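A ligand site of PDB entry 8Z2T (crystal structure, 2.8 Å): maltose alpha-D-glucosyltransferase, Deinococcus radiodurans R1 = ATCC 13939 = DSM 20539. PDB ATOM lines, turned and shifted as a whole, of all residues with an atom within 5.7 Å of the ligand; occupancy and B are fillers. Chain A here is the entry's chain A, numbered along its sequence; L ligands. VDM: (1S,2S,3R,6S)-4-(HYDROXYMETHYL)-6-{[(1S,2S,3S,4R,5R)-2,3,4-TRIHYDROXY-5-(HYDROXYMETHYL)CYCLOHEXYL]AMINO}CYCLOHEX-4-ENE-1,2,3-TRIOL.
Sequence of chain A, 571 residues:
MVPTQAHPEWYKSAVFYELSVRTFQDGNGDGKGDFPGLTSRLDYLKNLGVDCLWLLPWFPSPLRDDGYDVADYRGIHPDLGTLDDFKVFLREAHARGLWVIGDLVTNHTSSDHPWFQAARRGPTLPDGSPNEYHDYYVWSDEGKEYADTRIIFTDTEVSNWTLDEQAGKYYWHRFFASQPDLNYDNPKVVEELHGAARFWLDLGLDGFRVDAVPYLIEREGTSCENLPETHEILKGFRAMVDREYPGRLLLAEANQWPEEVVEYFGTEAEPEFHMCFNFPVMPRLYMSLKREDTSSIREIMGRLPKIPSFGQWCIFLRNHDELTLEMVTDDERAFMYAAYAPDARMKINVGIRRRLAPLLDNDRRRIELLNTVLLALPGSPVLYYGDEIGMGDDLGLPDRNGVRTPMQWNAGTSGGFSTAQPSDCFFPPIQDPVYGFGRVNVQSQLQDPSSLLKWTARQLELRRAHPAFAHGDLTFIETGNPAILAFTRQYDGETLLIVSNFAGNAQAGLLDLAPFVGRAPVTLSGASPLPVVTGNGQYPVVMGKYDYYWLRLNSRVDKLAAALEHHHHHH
O4' of the ligand lies within hydrogen-bond range of OD2 of Asp 65, at 2.6 Å.
The side-chain carboxylate (OE1) of Glu 322 lies within hydrogen-bond range of an oxygen (O3) of the ligand, at 2.7 Å.
The side-chain carboxylate of Glu 326 sits at hydrogen-bond distance from an oxygen (O7) of the ligand.
A nitrogen (N1') of the ligand is in salt-bridge range of the side-chain carboxylate (OD2) of Asp 321, at 3.0 Å.
OE2 of Glu 253 lies within salt-bridge range of N1' of the ligand, 2.8 Å away.
An oxygen (O2') of the ligand is in hydrogen-bond range of a ring nitrogen (NE2) of His 320, at 2.9 Å.
O4' of the ligand sits at hydrogen-bond distance from NH1 of Arg 400, at 2.9 Å.
O7' of the ligand sits at hydrogen-bond distance from NE2 of His 108, 3.1 Å away.
NE2 of Gln 179 lies within hydrogen-bond range of O7' of the ligand, 3.1 Å away.
An oxygen (O2') of the ligand is in hydrogen-bond range of the guanidinium group (NH2) of Arg 209, at 3.3 Å.
The side-chain amide nitrogen (NE2) of Gln 179 sits at hydrogen-bond distance from the side-chain carboxylate (OD2) of Asp 65, 2.8 Å away.
The side-chain carboxylate (OD1) of Asp 321 is in salt-bridge range of the guanidinium group (NH1) of Arg 400.
The side-chain carboxylate of Asp 321 is in salt-bridge range of the guanidinium group of Arg 404, at 3.3 Å.
The side-chain carboxylate (OE2) of Glu 253 lies within salt-bridge range of the guanidinium group (NH1) of Arg 209.
A ring nitrogen (NE2) of His 320 lies within hydrogen-bond range of the side-chain hydroxyl (OH) of Tyr 68, 3.0 Å away.
OD1 of Asp 211 is in salt-bridge range of NH2 of Arg 209 (3.0 Å).
OG1 of Thr 324 sits at hydrogen-bond distance from ND2 of Asn 255 (3.2 Å).
The guanidinium group (NH2) of Arg 150 sits at hydrogen-bond distance from the side-chain hydroxyl (OH) of Tyr 215, at 2.9 Å.
Merely in contact with the ligand: Tyr 68, Phe 153, Phe 175, Asp 211, Tyr 215, Asn 255, Thr 324 and Arg 404.
Hydrophobic or aromatic side chains within 4 Å of the ligand: Tyr 68, His 108, Phe 153, Phe 175 and His 320.
18 residues have an atom within 4 Å of the ligand: Asp 65, Tyr 68, His 108, Phe 153, Phe 175, Gln 179, Arg 209, Asp 211, Tyr 215, Glu 253, Asn 255, His 320, Asp 321, Glu 322, Thr 324, Glu 326, Arg 400 and Arg 404.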
ATOM      1  N   ASP A  65     -13.950  19.256 -11.876  1.00  0.00           N
ATOM      2  CA  ASP A  65     -12.937  18.404 -11.264  1.00  0.00           C
ATOM      3  C   ASP A  65     -11.615  18.499 -12.028  1.00  0.00           C
ATOM      4  O   ASP A  65     -10.942  17.497 -12.248  1.00  0.00           O
ATOM      5  CB  ASP A  65     -13.399  16.962 -11.215  1.00  0.00           C
ATOM      6  CG  ASP A  65     -12.603  16.124 -10.220  1.00  0.00           C
ATOM      7  OD1 ASP A  65     -11.846  16.713  -9.411  1.00  0.00           O
ATOM      8  OD2 ASP A  65     -12.738  14.887 -10.241  1.00  0.00           O
ATOM      9  N   TYR A  68     -11.091  16.011 -14.926  1.00  0.00           N
ATOM     10  CA  TYR A  68     -11.589  14.652 -14.716  1.00  0.00           C
ATOM     11  C   TYR A  68     -13.101  14.565 -14.867  1.00  0.00           C
ATOM     12  O   TYR A  68     -13.660  13.470 -14.707  1.00  0.00           O
ATOM     13  CB  TYR A  68     -11.173  14.132 -13.320  1.00  0.00           C
ATOM     14  CG  TYR A  68      -9.739  13.691 -13.267  1.00  0.00           C
ATOM     15  CD1 TYR A  68      -9.351  12.437 -13.759  1.00  0.00           C
ATOM     16  CD2 TYR A  68      -8.740  14.535 -12.766  1.00  0.00           C
ATOM     17  CE1 TYR A  68      -8.039  12.033 -13.736  1.00  0.00           C
ATOM     18  CE2 TYR A  68      -7.421  14.139 -12.744  1.00  0.00           C
ATOM     19  CZ  TYR A  68      -7.080  12.882 -13.231  1.00  0.00           C
ATOM     20  OH  TYR A  68      -5.777  12.471 -13.221  1.00  0.00           O
ATOM     21  N   ASP A  69     -13.764  15.711 -15.138  1.00  0.00           N
ATOM     22  CA  ASP A  69     -15.160  15.773 -15.578  1.00  0.00           C
ATOM     23  C   ASP A  69     -15.153  16.032 -17.092  1.00  0.00           C
ATOM     24  O   ASP A  69     -15.077  17.164 -17.571  1.00  0.00           O
ATOM     25  CB  ASP A  69     -15.956  16.818 -14.774  1.00  0.00           C
ATOM     26  CG  ASP A  69     -15.444  18.269 -14.909  1.00  0.00           C
ATOM     27  OD1 ASP A  69     -14.217  18.526 -15.006  1.00  0.00           O
ATOM     28  OD2 ASP A  69     -16.315  19.184 -14.878  1.00  0.00           O
ATOM     29  N   VAL A 105     -10.622   8.566 -18.274  1.00  0.00           N
ATOM     30  CA  VAL A 105     -11.648   8.663 -17.235  1.00  0.00           C
ATOM     31  C   VAL A 105     -12.826   7.803 -17.692  1.00  0.00           C
ATOM     32  O   VAL A 105     -13.522   8.162 -18.648  1.00  0.00           O
ATOM     33  CB  VAL A 105     -12.091  10.107 -16.982  1.00  0.00           C
ATOM     34  CG1 VAL A 105     -12.890  10.176 -15.689  1.00  0.00           C
ATOM     35  CG2 VAL A 105     -10.910  11.045 -16.950  1.00  0.00           C
ATOM     36  N   HIS A 108     -17.162   7.703 -15.254  1.00  0.00           N
ATOM     37  CA  HIS A 108     -18.112   8.797 -15.251  1.00  0.00           C
ATOM     38  C   HIS A 108     -17.716   9.807 -16.317  1.00  0.00           C
ATOM     39  O   HIS A 108     -16.566   9.819 -16.784  1.00  0.00           O
ATOM     40  CB  HIS A 108     -18.144   9.452 -13.875  1.00  0.00           C
ATOM     41  CG  HIS A 108     -16.781   9.836 -13.378  1.00  0.00           C
ATOM     42  ND1 HIS A 108     -15.968   8.972 -12.686  1.00  0.00           N
ATOM     43  CD2 HIS A 108     -16.085  10.993 -13.514  1.00  0.00           C
ATOM     44  CE1 HIS A 108     -14.826   9.580 -12.395  1.00  0.00           C
ATOM     45  NE2 HIS A 108     -14.876  10.804 -12.880  1.00  0.00           N
ATOM     46  N   ARG A 150     -19.927   3.465   0.171  1.00  0.00           N
ATOM     47  CA  ARG A 150     -19.025   4.503   0.666  1.00  0.00           C
ATOM     48  C   ARG A 150     -19.097   5.749  -0.201  1.00  0.00           C
ATOM     49  O   ARG A 150     -19.196   5.665  -1.433  1.00  0.00           O
ATOM     50  CB  ARG A 150     -17.599   3.942   0.689  1.00  0.00           C
ATOM     51  CG  ARG A 150     -16.550   4.819   1.337  1.00  0.00           C
ATOM     52  CD  ARG A 150     -15.304   3.994   1.627  1.00  0.00           C
ATOM     53  NE  ARG A 150     -14.671   3.517   0.408  1.00  0.00           N
ATOM     54  CZ  ARG A 150     -13.942   4.287  -0.388  1.00  0.00           C
ATOM     55  NH1 ARG A 150     -13.767   5.580  -0.118  1.00  0.00           N
ATOM     56  NH2 ARG A 150     -13.381   3.757  -1.471  1.00  0.00           N
ATOM     57  N   ILE A 152     -17.052   8.901  -1.540  1.00  0.00           N
ATOM     58  CA  ILE A 152     -15.643   9.247  -1.672  1.00  0.00           C
ATOM     59  C   ILE A 152     -15.410  10.724  -1.340  1.00  0.00           C
ATOM     60  O   ILE A 152     -14.605  11.047  -0.463  1.00  0.00           O
ATOM     61  CB  ILE A 152     -15.118   8.877  -3.077  1.00  0.00           C
ATOM     62  CG1 ILE A 152     -15.146   7.358  -3.240  1.00  0.00           C
ATOM     63  CG2 ILE A 152     -13.695   9.370  -3.266  1.00  0.00           C
ATOM     64  CD1 ILE A 152     -14.910   6.875  -4.660  1.00  0.00           C
ATOM     65  N   PHE A 153     -16.154  11.627  -1.971  1.00  0.00           N
ATOM     66  CA  PHE A 153     -15.970  13.061  -1.735  1.00  0.00           C
ATOM     67  C   PHE A 153     -16.870  13.531  -0.580  1.00  0.00           C
ATOM     68  O   PHE A 153     -17.777  14.351  -0.760  1.00  0.00           O
ATOM     69  CB  PHE A 153     -16.239  13.838  -3.022  1.00  0.00           C
ATOM     70  CG  PHE A 153     -15.166  13.668  -4.084  1.00  0.00           C
ATOM     71  CD1 PHE A 153     -13.987  13.002  -3.798  1.00  0.00           C
ATOM     72  CD2 PHE A 153     -15.361  14.182  -5.362  1.00  0.00           C
ATOM     73  CE1 PHE A 153     -12.997  12.845  -4.785  1.00  0.00           C
ATOM     74  CE2 PHE A 153     -14.384  14.035  -6.359  1.00  0.00           C
ATOM     75  CZ  PHE A 153     -13.195  13.362  -6.054  1.00  0.00           C
ATOM     76  N   PHE A 175     -18.371  10.254  -7.591  1.00  0.00           N
ATOM     77  CA  PHE A 175     -17.620  11.453  -7.285  1.00  0.00           C
ATOM     78  C   PHE A 175     -18.549  12.668  -7.270  1.00  0.00           C
ATOM     79  O   PHE A 175     -19.676  12.567  -6.786  1.00  0.00           O
ATOM     80  CB  PHE A 175     -16.465  11.585  -8.281  1.00  0.00           C
ATOM     81  CG  PHE A 175     -15.573  10.398  -8.252  1.00  0.00           C
ATOM     82  CD1 PHE A 175     -14.591  10.277  -7.271  1.00  0.00           C
ATOM     83  CD2 PHE A 175     -15.765   9.348  -9.139  1.00  0.00           C
ATOM     84  CE1 PHE A 175     -13.786   9.156  -7.188  1.00  0.00           C
ATOM     85  CE2 PHE A 175     -14.976   8.212  -9.069  1.00  0.00           C
ATOM     86  CZ  PHE A 175     -13.972   8.112  -8.098  1.00  0.00           C
ATOM     87  N   GLN A 179     -20.594  14.771 -12.179  1.00  0.00           N
ATOM     88  CA  GLN A 179     -19.752  13.695 -12.690  1.00  0.00           C
ATOM     89  C   GLN A 179     -20.566  12.407 -12.660  1.00  0.00           C
ATOM     90  O   GLN A 179     -20.187  11.436 -11.989  1.00  0.00           O
ATOM     91  CB  GLN A 179     -18.485  13.546 -11.852  1.00  0.00           C
ATOM     92  CG  GLN A 179     -17.284  14.308 -12.366  1.00  0.00           C
ATOM     93  CD  GLN A 179     -16.084  14.252 -11.395  1.00  0.00           C
ATOM     94  OE1 GLN A 179     -16.255  14.222 -10.168  1.00  0.00           O
ATOM     95  NE2 GLN A 179     -14.878  14.244 -11.945  1.00  0.00           N
ATOM     96  N   ARG A 209      -3.215   5.845 -18.198  1.00  0.00           N
ATOM     97  CA  ARG A 209      -3.580   5.680 -16.800  1.00  0.00           C
ATOM     98  C   ARG A 209      -5.096   5.569 -16.739  1.00  0.00           C
ATOM     99  O   ARG A 209      -5.805   6.453 -17.234  1.00  0.00           O
ATOM    100  CB  ARG A 209      -3.107   6.836 -15.911  1.00  0.00           C
ATOM    101  CG  ARG A 209      -3.048   6.366 -14.467  1.00  0.00           C
ATOM    102  CD  ARG A 209      -3.289   7.393 -13.389  1.00  0.00           C
ATOM    103  NE  ARG A 209      -4.633   7.969 -13.394  1.00  0.00           N
ATOM    104  CZ  ARG A 209      -5.238   8.469 -12.319  1.00  0.00           C
ATOM    105  NH1 ARG A 209      -4.682   8.444 -11.117  1.00  0.00           N
ATOM    106  NH2 ARG A 209      -6.444   9.013 -12.460  1.00  0.00           N
ATOM    107  N   ASP A 211      -8.515   5.551 -14.763  1.00  0.00           N
ATOM    108  CA  ASP A 211      -8.907   6.284 -13.578  1.00  0.00           C
ATOM    109  C   ASP A 211     -10.072   5.591 -12.879  1.00  0.00           C
ATOM    110  O   ASP A 211     -11.022   5.135 -13.530  1.00  0.00           O
ATOM    111  CB  ASP A 211      -9.276   7.703 -14.026  1.00  0.00           C
ATOM    112  CG  ASP A 211     -10.047   8.481 -12.994  1.00  0.00           C
ATOM    113  OD1 ASP A 211      -9.394   8.942 -12.036  1.00  0.00           O
ATOM    114  OD2 ASP A 211     -11.294   8.645 -13.178  1.00  0.00           O
ATOM    115  N   ALA A 212      -9.981   5.488 -11.539  1.00  0.00           N
ATOM    116  CA  ALA A 212     -11.099   5.101 -10.676  1.00  0.00           C
ATOM    117  C   ALA A 212     -11.686   3.743 -11.040  1.00  0.00           C
ATOM    118  O   ALA A 212     -12.887   3.520 -10.864  1.00  0.00           O
ATOM    119  CB  ALA A 212     -12.219   6.156 -10.709  1.00  0.00           C
ATOM    120  N   TYR A 215     -14.693   1.253  -9.358  1.00  0.00           N
ATOM    121  CA  TYR A 215     -16.067   1.690  -9.110  1.00  0.00           C
ATOM    122  C   TYR A 215     -16.958   1.584 -10.361  1.00  0.00           C
ATOM    123  O   TYR A 215     -17.995   2.242 -10.471  1.00  0.00           O
ATOM    124  CB  TYR A 215     -16.080   3.109  -8.530  1.00  0.00           C
ATOM    125  CG  TYR A 215     -15.127   3.325  -7.383  1.00  0.00           C
ATOM    126  CD1 TYR A 215     -15.211   2.563  -6.215  1.00  0.00           C
ATOM    127  CD2 TYR A 215     -14.129   4.292  -7.461  1.00  0.00           C
ATOM    128  CE1 TYR A 215     -14.295   2.752  -5.165  1.00  0.00           C
ATOM    129  CE2 TYR A 215     -13.222   4.499  -6.421  1.00  0.00           C
ATOM    130  CZ  TYR A 215     -13.308   3.726  -5.262  1.00  0.00           C
ATOM    131  OH  TYR A 215     -12.398   3.943  -4.236  1.00  0.00           O
ATOM    132  N   GLU A 253      -5.435   2.857 -11.526  1.00  0.00           N
ATOM    133  CA  GLU A 253      -5.542   3.561 -10.256  1.00  0.00           C
ATOM    134  C   GLU A 253      -6.536   2.789  -9.377  1.00  0.00           C
ATOM    135  O   GLU A 253      -7.756   2.949  -9.503  1.00  0.00           O
ATOM    136  CB  GLU A 253      -5.961   5.002 -10.482  1.00  0.00           C
ATOM    137  CG  GLU A 253      -5.758   5.851  -9.258  1.00  0.00           C
ATOM    138  CD  GLU A 253      -6.931   6.737  -8.968  1.00  0.00           C
ATOM    139  OE1 GLU A 253      -8.005   6.509  -9.570  1.00  0.00           O
ATOM    140  OE2 GLU A 253      -6.783   7.668  -8.138  1.00  0.00           O
ATOM    141  N   ASN A 255      -6.803   2.112  -5.511  1.00  0.00           N
ATOM    142  CA  ASN A 255      -6.434   2.207  -4.111  1.00  0.00           C
ATOM    143  C   ASN A 255      -7.378   1.307  -3.337  1.00  0.00           C
ATOM    144  O   ASN A 255      -8.449   1.730  -2.911  1.00  0.00           O
ATOM    145  CB  ASN A 255      -6.512   3.631  -3.617  1.00  0.00           C
ATOM    146  CG  ASN A 255      -6.137   3.737  -2.173  1.00  0.00           C
ATOM    147  OD1 ASN A 255      -5.391   2.900  -1.644  1.00  0.00           O
ATOM    148  ND2 ASN A 255      -6.667   4.742  -1.518  1.00  0.00           N
ATOM    149  N   PHE A 279      -0.607   1.707  -4.204  1.00  0.00           N
ATOM    150  CA  PHE A 279      -1.248   2.455  -3.128  1.00  0.00           C
ATOM    151  C   PHE A 279      -0.995   1.867  -1.743  1.00  0.00           C
ATOM    152  O   PHE A 279      -0.862   2.655  -0.789  1.00  0.00           O
ATOM    153  CB  PHE A 279      -2.756   2.558  -3.379  1.00  0.00           C
ATOM    154  CG  PHE A 279      -3.141   3.749  -4.187  1.00  0.00           C
ATOM    155  CD1 PHE A 279      -3.157   5.011  -3.599  1.00  0.00           C
ATOM    156  CD2 PHE A 279      -3.472   3.619  -5.513  1.00  0.00           C
ATOM    157  CE1 PHE A 279      -3.486   6.116  -4.331  1.00  0.00           C
ATOM    158  CE2 PHE A 279      -3.817   4.722  -6.263  1.00  0.00           C
ATOM    159  CZ  PHE A 279      -3.820   5.974  -5.666  1.00  0.00           C
ATOM    160  N   HIS A 320      -1.356  14.127  -7.661  1.00  0.00           N
ATOM    161  CA  HIS A 320      -2.199  15.325  -7.752  1.00  0.00           C
ATOM    162  C   HIS A 320      -3.406  15.277  -6.819  1.00  0.00           C
ATOM    163  O   HIS A 320      -4.135  16.278  -6.725  1.00  0.00           O
ATOM    164  CB  HIS A 320      -2.660  15.504  -9.207  1.00  0.00           C
ATOM    165  CG  HIS A 320      -3.531  14.394  -9.699  1.00  0.00           C
ATOM    166  ND1 HIS A 320      -3.059  13.129  -9.933  1.00  0.00           N
ATOM    167  CD2 HIS A 320      -4.864  14.359  -9.940  1.00  0.00           C
ATOM    168  CE1 HIS A 320      -4.059  12.352 -10.322  1.00  0.00           C
ATOM    169  NE2 HIS A 320      -5.167  13.078 -10.337  1.00  0.00           N
ATOM    170  N   ASP A 321      -3.659  14.158  -6.145  1.00  0.00           N
ATOM    171  CA  ASP A 321      -4.752  14.040  -5.207  1.00  0.00           C
ATOM    172  C   ASP A 321      -4.237  14.277  -3.796  1.00  0.00           C
ATOM    173  O   ASP A 321      -3.090  14.705  -3.576  1.00  0.00           O
ATOM    174  CB  ASP A 321      -5.396  12.674  -5.307  1.00  0.00           C
ATOM    175  CG  ASP A 321      -6.214  12.490  -6.580  1.00  0.00           C
ATOM    176  OD1 ASP A 321      -6.857  13.452  -7.052  1.00  0.00           O
ATOM    177  OD2 ASP A 321      -6.210  11.339  -7.098  1.00  0.00           O
ATOM    178  N   GLU A 322      -5.063  13.981  -2.819  1.00  0.00           N
ATOM    179  CA  GLU A 322      -4.577  14.037  -1.471  1.00  0.00           C
ATOM    180  C   GLU A 322      -3.770  12.766  -1.151  1.00  0.00           C
ATOM    181  O   GLU A 322      -3.806  11.781  -1.893  1.00  0.00           O
ATOM    182  CB  GLU A 322      -5.745  14.260  -0.502  1.00  0.00           C
ATOM    183  CG  GLU A 322      -6.524  13.014  -0.107  1.00  0.00           C
ATOM    184  CD  GLU A 322      -7.334  12.423  -1.234  1.00  0.00           C
ATOM    185  OE1 GLU A 322      -7.570  13.166  -2.210  1.00  0.00           O
ATOM    186  OE2 GLU A 322      -7.728  11.231  -1.152  1.00  0.00           O
ATOM    187  N   THR A 324      -3.823   9.654   0.421  1.00  0.00           N
ATOM    188  CA  THR A 324      -5.076   9.009   0.780  1.00  0.00           C
ATOM    189  C   THR A 324      -4.951   8.136   2.018  1.00  0.00           C
ATOM    190  O   THR A 324      -4.011   7.352   2.165  1.00  0.00           O
ATOM    191  CB  THR A 324      -5.623   8.176  -0.390  1.00  0.00           C
ATOM    192  OG1 THR A 324      -6.795   7.488   0.053  1.00  0.00           O
ATOM    193  CG2 THR A 324      -4.576   7.160  -0.937  1.00  0.00           C
ATOM    194  N   GLU A 326      -7.724   6.177   2.837  1.00  0.00           N
ATOM    195  CA  GLU A 326      -8.900   5.318   2.711  1.00  0.00           C
ATOM    196  C   GLU A 326      -8.598   3.871   3.107  1.00  0.00           C
ATOM    197  O   GLU A 326      -9.459   3.210   3.672  1.00  0.00           O
ATOM    198  CB  GLU A 326      -9.436   5.380   1.289  1.00  0.00           C
ATOM    199  CG  GLU A 326     -10.022   6.760   0.876  1.00  0.00           C
ATOM    200  CD  GLU A 326     -10.168   6.943  -0.653  1.00  0.00           C
ATOM    201  OE1 GLU A 326      -9.202   7.424  -1.293  1.00  0.00           O
ATOM    202  OE2 GLU A 326     -11.232   6.586  -1.216  1.00  0.00           O
ATOM    203  N   ARG A 400      -8.242  19.771  -4.186  1.00  0.00           N
ATOM    204  CA  ARG A 400      -6.882  19.269  -4.211  1.00  0.00           C
ATOM    205  C   ARG A 400      -6.004  20.124  -5.100  1.00  0.00           C
ATOM    206  O   ARG A 400      -4.898  19.715  -5.459  1.00  0.00           O
ATOM    207  CB  ARG A 400      -6.886  17.818  -4.673  1.00  0.00           C
ATOM    208  CG  ARG A 400      -7.580  16.907  -3.722  1.00  0.00           C
ATOM    209  CD  ARG A 400      -8.342  15.844  -4.434  1.00  0.00           C
ATOM    210  NE  ARG A 400      -9.390  16.427  -5.252  1.00  0.00           N
ATOM    211  CZ  ARG A 400     -10.058  15.756  -6.176  1.00  0.00           C
ATOM    212  NH1 ARG A 400      -9.704  14.533  -6.522  1.00  0.00           N
ATOM    213  NH2 ARG A 400     -11.111  16.317  -6.760  1.00  0.00           N
ATOM    214  N   ARG A 404      -1.377  21.594  -7.258  1.00  0.00           N
ATOM    215  CA  ARG A 404      -1.421  21.632  -8.715  1.00  0.00           C
ATOM    216  C   ARG A 404      -0.952  22.985  -9.243  1.00  0.00           C
ATOM    217  O   ARG A 404      -1.201  23.308 -10.409  1.00  0.00           O
ATOM    218  CB  ARG A 404      -2.841  21.315  -9.203  1.00  0.00           C
ATOM    219  CG  ARG A 404      -3.201  19.857  -8.969  1.00  0.00           C
ATOM    220  CD  ARG A 404      -4.647  19.558  -9.211  1.00  0.00           C
ATOM    221  NE  ARG A 404      -5.011  18.308  -8.548  1.00  0.00           N
ATOM    222  CZ  ARG A 404      -6.144  17.649  -8.738  1.00  0.00           C
ATOM    223  NH1 ARG A 404      -7.050  18.066  -9.609  1.00  0.00           N
ATOM    224  NH2 ARG A 404      -6.362  16.516  -8.067  1.00  0.00           N
HETATM  225  O7  VDM L   1      -9.303   6.056  -3.627  1.00  0.00           O
HETATM  226  C7  VDM L   1      -8.106   6.638  -4.114  1.00  0.00           C
HETATM  227  C5  VDM L   1      -8.431   7.928  -4.784  1.00  0.00           C
HETATM  228  C6  VDM L   1      -9.057   7.919  -5.957  1.00  0.00           C
HETATM  229  C4  VDM L   1      -8.365   9.132  -3.901  1.00  0.00           C
HETATM  230  O4  VDM L   1      -7.108   9.239  -3.283  1.00  0.00           O
HETATM  231  C3  VDM L   1      -8.644  10.369  -4.715  1.00  0.00           C
HETATM  232  O3  VDM L   1      -8.816  11.507  -3.898  1.00  0.00           O
HETATM  233  C2  VDM L   1      -9.902  10.179  -5.544  1.00  0.00           C
HETATM  234  O2  VDM L   1     -10.363  11.386  -6.117  1.00  0.00           O
HETATM  235  C1  VDM L   1      -9.594   9.152  -6.639  1.00  0.00           C
HETATM  236  N1' VDM L   1      -8.638   9.712  -7.619  1.00  0.00           N
HETATM  237  C1' VDM L   1      -8.980   9.744  -9.052  1.00  0.00           C
HETATM  238  C2' VDM L   1      -8.346  10.906  -9.797  1.00  0.00           C
HETATM  239  O2' VDM L   1      -6.941  10.870  -9.717  1.00  0.00           O
HETATM  240  C6' VDM L   1     -10.473   9.769  -9.428  1.00  0.00           C
HETATM  241  C5' VDM L   1     -11.210  11.112  -9.526  1.00  0.00           C
HETATM  242  C7' VDM L   1     -12.097  10.967 -10.762  1.00  0.00           C
HETATM  243  O7' VDM L   1     -12.723  12.179 -11.166  1.00  0.00           O
HETATM  244  C4' VDM L   1     -10.355  12.389  -9.671  1.00  0.00           C
HETATM  245  O4' VDM L   1     -10.905  13.485  -8.976  1.00  0.00           O
HETATM  246  C3' VDM L   1      -8.903  12.211  -9.247  1.00  0.00           C
HETATM  247  O3' VDM L   1      -8.084  13.292  -9.646  1.00  0.00           O
